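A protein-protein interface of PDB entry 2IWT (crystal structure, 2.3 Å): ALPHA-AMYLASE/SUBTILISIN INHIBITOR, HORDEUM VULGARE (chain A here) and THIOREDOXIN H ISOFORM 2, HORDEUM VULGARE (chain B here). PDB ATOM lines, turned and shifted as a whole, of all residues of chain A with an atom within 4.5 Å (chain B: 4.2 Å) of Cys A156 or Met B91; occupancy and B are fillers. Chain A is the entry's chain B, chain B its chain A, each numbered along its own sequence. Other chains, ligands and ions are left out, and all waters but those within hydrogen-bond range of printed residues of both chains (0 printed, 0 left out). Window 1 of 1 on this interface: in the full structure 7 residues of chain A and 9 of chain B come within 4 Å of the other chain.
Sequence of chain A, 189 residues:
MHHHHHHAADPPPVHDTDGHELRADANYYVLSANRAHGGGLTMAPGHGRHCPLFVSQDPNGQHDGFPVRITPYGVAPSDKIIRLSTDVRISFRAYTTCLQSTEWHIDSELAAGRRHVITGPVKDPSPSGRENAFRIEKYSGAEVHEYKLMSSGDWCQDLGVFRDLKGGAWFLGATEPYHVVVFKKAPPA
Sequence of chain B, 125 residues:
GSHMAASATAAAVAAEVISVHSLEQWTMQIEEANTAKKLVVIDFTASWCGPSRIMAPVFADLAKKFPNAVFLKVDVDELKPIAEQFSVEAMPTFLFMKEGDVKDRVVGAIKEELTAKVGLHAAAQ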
ATOM      1  N   MET A 150       0.705  -8.850   3.043  1.00  0.00           N
ATOM      2  CA  MET A 150      -0.350  -8.084   2.378  1.00  0.00           C
ATOM      3  C   MET A 150      -0.308  -6.574   2.648  1.00  0.00           C
ATOM      4  O   MET A 150       0.084  -6.119   3.729  1.00  0.00           O
ATOM      5  CB  MET A 150      -1.733  -8.605   2.802  1.00  0.00           C
ATOM      6  CG  MET A 150      -2.041 -10.072   2.461  1.00  0.00           C
ATOM      7  SD  MET A 150      -3.836 -10.479   2.517  1.00  0.00           S
ATOM      8  CE  MET A 150      -4.438  -9.623   1.086  1.00  0.00           C
ATOM      9  N   SER A 151      -0.696  -5.800   1.644  1.00  0.00           N
ATOM     10  CA  SER A 151      -0.777  -4.348   1.795  1.00  0.00           C
ATOM     11  C   SER A 151      -2.166  -4.183   2.420  1.00  0.00           C
ATOM     12  O   SER A 151      -3.133  -4.750   1.922  1.00  0.00           O
ATOM     13  CB  SER A 151      -0.741  -3.663   0.422  1.00  0.00           C
ATOM     14  OG  SER A 151      -0.751  -2.252   0.532  1.00  0.00           O
ATOM     15  N   TRP A 155      -6.501  -0.484   1.068  1.00  0.00           N
ATOM     16  CA  TRP A 155      -6.992  -1.666   0.353  1.00  0.00           C
ATOM     17  C   TRP A 155      -6.321  -2.924   0.922  1.00  0.00           C
ATOM     18  O   TRP A 155      -5.417  -2.827   1.755  1.00  0.00           O
ATOM     19  CB  TRP A 155      -6.681  -1.535  -1.146  1.00  0.00           C
ATOM     20  CG  TRP A 155      -5.203  -1.582  -1.488  1.00  0.00           C
ATOM     21  CD1 TRP A 155      -4.148  -1.521  -0.610  1.00  0.00           C
ATOM     22  CD2 TRP A 155      -4.617  -1.683  -2.796  1.00  0.00           C
ATOM     23  NE1 TRP A 155      -2.952  -1.579  -1.290  1.00  0.00           N
ATOM     24  CE2 TRP A 155      -3.208  -1.679  -2.630  1.00  0.00           C
ATOM     25  CE3 TRP A 155      -5.142  -1.776  -4.092  1.00  0.00           C
ATOM     26  CZ2 TRP A 155      -2.318  -1.766  -3.710  1.00  0.00           C
ATOM     27  CZ3 TRP A 155      -4.254  -1.864  -5.179  1.00  0.00           C
ATOM     28  CH2 TRP A 155      -2.859  -1.858  -4.977  1.00  0.00           C
ATOM     29  N   CYS A 156      -6.762  -4.104   0.493  1.00  0.00           N
ATOM     30  CA  CYS A 156      -6.146  -5.355   0.943  1.00  0.00           C
ATOM     31  C   CYS A 156      -5.706  -6.031  -0.342  1.00  0.00           C
ATOM     32  O   CYS A 156      -6.519  -6.313  -1.211  1.00  0.00           O
ATOM     33  CB  CYS A 156      -7.160  -6.206   1.712  1.00  0.00           C
ATOM     34  SG  CYS A 156      -7.819  -5.347   3.199  1.00  0.00           S
ATOM     35  N   GLN A 157      -4.407  -6.265  -0.481  1.00  0.00           N
ATOM     36  CA  GLN A 157      -3.856  -6.868  -1.689  1.00  0.00           C
ATOM     37  C   GLN A 157      -2.628  -7.726  -1.314  1.00  0.00           C
ATOM     38  O   GLN A 157      -1.828  -7.289  -0.497  1.00  0.00           O
ATOM     39  CB  GLN A 157      -3.415  -5.750  -2.644  1.00  0.00           C
ATOM     40  CG  GLN A 157      -2.394  -6.185  -3.690  1.00  0.00           C
ATOM     41  CD  GLN A 157      -3.014  -6.430  -5.038  1.00  0.00           C
ATOM     42  OE1 GLN A 157      -3.569  -5.510  -5.632  1.00  0.00           O
ATOM     43  NE2 GLN A 157      -2.919  -7.667  -5.541  1.00  0.00           N
ATOM     44  N   PHE B  44     -16.783  -4.896  -5.161  1.00  0.00           N
ATOM     45  CA  PHE B  44     -16.217  -6.222  -4.834  1.00  0.00           C
ATOM     46  C   PHE B  44     -15.604  -6.071  -3.451  1.00  0.00           C
ATOM     47  O   PHE B  44     -14.622  -5.337  -3.256  1.00  0.00           O
ATOM     48  CB  PHE B  44     -15.153  -6.622  -5.851  1.00  0.00           C
ATOM     49  CG  PHE B  44     -15.723  -6.979  -7.197  1.00  0.00           C
ATOM     50  CD1 PHE B  44     -16.052  -8.294  -7.509  1.00  0.00           C
ATOM     51  CD2 PHE B  44     -15.987  -5.984  -8.133  1.00  0.00           C
ATOM     52  CE1 PHE B  44     -16.637  -8.613  -8.733  1.00  0.00           C
ATOM     53  CE2 PHE B  44     -16.569  -6.290  -9.358  1.00  0.00           C
ATOM     54  CZ  PHE B  44     -16.895  -7.609  -9.658  1.00  0.00           C
ATOM     55  N   THR B  45     -16.184  -6.790  -2.500  1.00  0.00           N
ATOM     56  CA  THR B  45     -15.798  -6.700  -1.101  1.00  0.00           C
ATOM     57  C   THR B  45     -15.202  -7.933  -0.434  1.00  0.00           C
ATOM     58  O   THR B  45     -15.127  -9.015  -1.012  1.00  0.00           O
ATOM     59  CB  THR B  45     -17.020  -6.317  -0.283  1.00  0.00           C
ATOM     60  OG1 THR B  45     -17.906  -7.447  -0.205  1.00  0.00           O
ATOM     61  CG2 THR B  45     -17.770  -5.164  -0.961  1.00  0.00           C
ATOM     62  N   ALA B  46     -14.811  -7.736   0.818  1.00  0.00           N
ATOM     63  CA  ALA B  46     -14.224  -8.764   1.659  1.00  0.00           C
ATOM     64  C   ALA B  46     -14.595  -8.361   3.091  1.00  0.00           C
ATOM     65  O   ALA B  46     -14.254  -7.265   3.523  1.00  0.00           O
ATOM     66  CB  ALA B  46     -12.698  -8.778   1.484  1.00  0.00           C
ATOM     67  N   TRP B  48     -13.443  -9.510   5.845  1.00  0.00           N
ATOM     68  CA  TRP B  48     -12.262  -9.493   6.724  1.00  0.00           C
ATOM     69  C   TRP B  48     -11.321  -8.320   6.418  1.00  0.00           C
ATOM     70  O   TRP B  48     -10.324  -8.118   7.099  1.00  0.00           O
ATOM     71  CB  TRP B  48     -11.495 -10.821   6.582  1.00  0.00           C
ATOM     72  CG  TRP B  48     -11.287 -11.223   5.139  1.00  0.00           C
ATOM     73  CD1 TRP B  48     -12.010 -12.162   4.419  1.00  0.00           C
ATOM     74  CD2 TRP B  48     -10.278 -10.729   4.246  1.00  0.00           C
ATOM     75  NE1 TRP B  48     -11.496 -12.282   3.144  1.00  0.00           N
ATOM     76  CE2 TRP B  48     -10.436 -11.421   3.008  1.00  0.00           C
ATOM     77  CE3 TRP B  48      -9.254  -9.771   4.366  1.00  0.00           C
ATOM     78  CZ2 TRP B  48      -9.599 -11.187   1.902  1.00  0.00           C
ATOM     79  CZ3 TRP B  48      -8.424  -9.541   3.272  1.00  0.00           C
ATOM     80  CH2 TRP B  48      -8.603 -10.252   2.049  1.00  0.00           C
ATOM     81  N   CYS B  49     -11.648  -7.538   5.392  1.00  0.00           N
ATOM     82  CA  CYS B  49     -10.790  -6.420   4.977  1.00  0.00           C
ATOM     83  C   CYS B  49     -11.240  -5.049   5.509  1.00  0.00           C
ATOM     84  O   CYS B  49     -12.256  -4.501   5.066  1.00  0.00           O
ATOM     85  CB  CYS B  49     -10.691  -6.401   3.440  1.00  0.00           C
ATOM     86  SG  CYS B  49      -9.790  -5.004   2.711  1.00  0.00           S
ATOM     87  N   PRO B  51     -10.376  -1.814   5.087  1.00  0.00           N
ATOM     88  CA  PRO B  51     -10.601  -0.815   4.034  1.00  0.00           C
ATOM     89  C   PRO B  51     -11.908  -1.040   3.293  1.00  0.00           C
ATOM     90  O   PRO B  51     -12.538  -0.092   2.824  1.00  0.00           O
ATOM     91  CB  PRO B  51      -9.410  -1.012   3.105  1.00  0.00           C
ATOM     92  CG  PRO B  51      -8.311  -1.359   4.058  1.00  0.00           C
ATOM     93  CD  PRO B  51      -8.980  -2.290   5.065  1.00  0.00           C
ATOM     94  N   VAL B  76     -15.899 -11.267  -2.621  1.00  0.00           N
ATOM     95  CA  VAL B  76     -14.948 -12.075  -3.384  1.00  0.00           C
ATOM     96  C   VAL B  76     -14.714 -13.477  -2.796  1.00  0.00           C
ATOM     97  O   VAL B  76     -14.310 -14.391  -3.520  1.00  0.00           O
ATOM     98  CB  VAL B  76     -13.583 -11.344  -3.580  1.00  0.00           C
ATOM     99  CG1 VAL B  76     -13.811  -9.987  -4.269  1.00  0.00           C
ATOM    100  CG2 VAL B  76     -12.891 -11.132  -2.229  1.00  0.00           C
ATOM    101  N   GLU B  89      -8.106  -7.909  -7.997  1.00  0.00           N
ATOM    102  CA  GLU B  89      -7.231  -8.533  -7.006  1.00  0.00           C
ATOM    103  C   GLU B  89      -7.125  -7.756  -5.692  1.00  0.00           C
ATOM    104  O   GLU B  89      -6.575  -8.265  -4.721  1.00  0.00           O
ATOM    105  CB  GLU B  89      -5.809  -8.741  -7.573  1.00  0.00           C
ATOM    106  CG  GLU B  89      -5.747  -9.444  -8.939  1.00  0.00           C
ATOM    107  CD  GLU B  89      -4.319  -9.778  -9.388  1.00  0.00           C
ATOM    108  OE1 GLU B  89      -3.383  -9.006  -9.062  1.00  0.00           O
ATOM    109  OE2 GLU B  89      -4.137 -10.805 -10.090  1.00  0.00           O
ATOM    110  N   ALA B  90      -7.636  -6.532  -5.653  1.00  0.00           N
ATOM    111  CA  ALA B  90      -7.583  -5.750  -4.427  1.00  0.00           C
ATOM    112  C   ALA B  90      -9.007  -5.463  -3.982  1.00  0.00           C
ATOM    113  O   ALA B  90      -9.914  -5.436  -4.811  1.00  0.00           O
ATOM    114  CB  ALA B  90      -6.822  -4.436  -4.669  1.00  0.00           C
ATOM    115  N   MET B  91      -9.209  -5.278  -2.677  1.00  0.00           N
ATOM    116  CA  MET B  91     -10.537  -4.977  -2.127  1.00  0.00           C
ATOM    117  C   MET B  91     -10.435  -3.770  -1.179  1.00  0.00           C
ATOM    118  O   MET B  91      -9.495  -3.668  -0.376  1.00  0.00           O
ATOM    119  CB  MET B  91     -11.109  -6.170  -1.333  1.00  0.00           C
ATOM    120  CG  MET B  91     -11.605  -7.370  -2.155  1.00  0.00           C
ATOM    121  SD  MET B  91     -10.231  -8.246  -2.952  1.00  0.00           S
ATOM    122  CE  MET B  91      -9.362  -8.875  -1.507  1.00  0.00           C
ATOM    123  N   PRO B  92     -11.401  -2.841  -1.260  1.00  0.00           N
ATOM    124  CA  PRO B  92     -12.526  -2.901  -2.196  1.00  0.00           C
ATOM    125  C   PRO B  92     -12.162  -2.413  -3.608  1.00  0.00           C
ATOM    126  O   PRO B  92     -11.188  -1.687  -3.796  1.00  0.00           O
ATOM    127  CB  PRO B  92     -13.565  -2.000  -1.526  1.00  0.00           C
ATOM    128  CG  PRO B  92     -12.694  -0.935  -0.907  1.00  0.00           C
ATOM    129  CD  PRO B  92     -11.579  -1.747  -0.287  1.00  0.00           C
ATOM    130  N   THR B  93     -12.931  -2.849  -4.600  1.00  0.00           N
ATOM    131  CA  THR B  93     -12.741  -2.412  -5.978  1.00  0.00           C
ATOM    132  C   THR B  93     -14.134  -2.135  -6.559  1.00  0.00           C
ATOM    133  O   THR B  93     -15.009  -2.999  -6.539  1.00  0.00           O
ATOM    134  CB  THR B  93     -12.022  -3.477  -6.848  1.00  0.00           C
ATOM    135  OG1 THR B  93     -10.612  -3.439  -6.595  1.00  0.00           O
ATOM    136  CG2 THR B  93     -12.242  -3.203  -8.326  1.00  0.00           C
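Of the printed residues of chain B, Cys A156 touches Trp B48 (3.9 Å), Cys B49 (2.1 Å), Pro B51 (3.8 Å), Ala B90 (3.4 Å) and Met B91 (2.9 Å). Met B91 touches just these residues of chain A: Trp A155 and Cys A156. Of the printed residues of chain A, Ala B90 touches Trp A155, Cys A156 and Gln A157. Printed residues of chain B within 4 Å of Trp A155: Pro B51, Ala B90 and Met B91. The nearest printed residue of chain B that does not touch Cys A156 is Glu B89 (4.02 Å). The nearest printed residue of chain A that does not touch Met B91 is Gln A157 (5.4 Å). The nearest printed residue of chain A that does not touch Glu B89 is Cys A156 (4.02 Å).
The side-chain sulfur (SG) of Cys B49 is disulfide-bonded to the side-chain sulfur (SG) of Cys A156, 2.1 Å away. The backbone carbonyl oxygen (O) of Met B91 sits at hydrogen-bond distance from the backbone NH (N) of Cys A156 (2.9 Å).
The side-chain hydroxyl (OG) of Ser A151 lies within hydrogen-bond range of the indole nitrogen (NE1) of Trp A155. The backbone NH of Ser A151 sits at hydrogen-bond distance from the backbone carbonyl oxygen of Gln A157 (2.8 Å). The side-chain hydroxyl (OG1) of Thr B93 lies within hydrogen-bond range of the backbone carbonyl oxygen (O) of Ala B90 (2.8 Å).
Hydrophobic or aromatic side chains of chain A within 4 Å of the printed part of chain B: Trp A155. Printed residues of chain B that touch a printed residue of chain A: Trp B48, Cys B49, Pro B51, Glu B89, Ala B90 and Met B91. Along chain B the printed residues that touch a printed residue of chain A span positions 48 to 91. Among the printed residues, 10 pairs touch across the chains. Among the printed residues, no Asp or Glu carboxylate lies within 4 Å of a Lys or Arg side-chain nitrogen of the other chain.
Among the printed residues, pairs that only touch across the chains: Trp A155 with Pro B51, Trp A155 with Ala B90, Trp A155 with Met B91, Cys A156 with Trp B48, Cys A156 with Pro B51, Cys A156 with Ala B90, Gln A157 with Glu B89 and Gln A157 with Ala B90.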
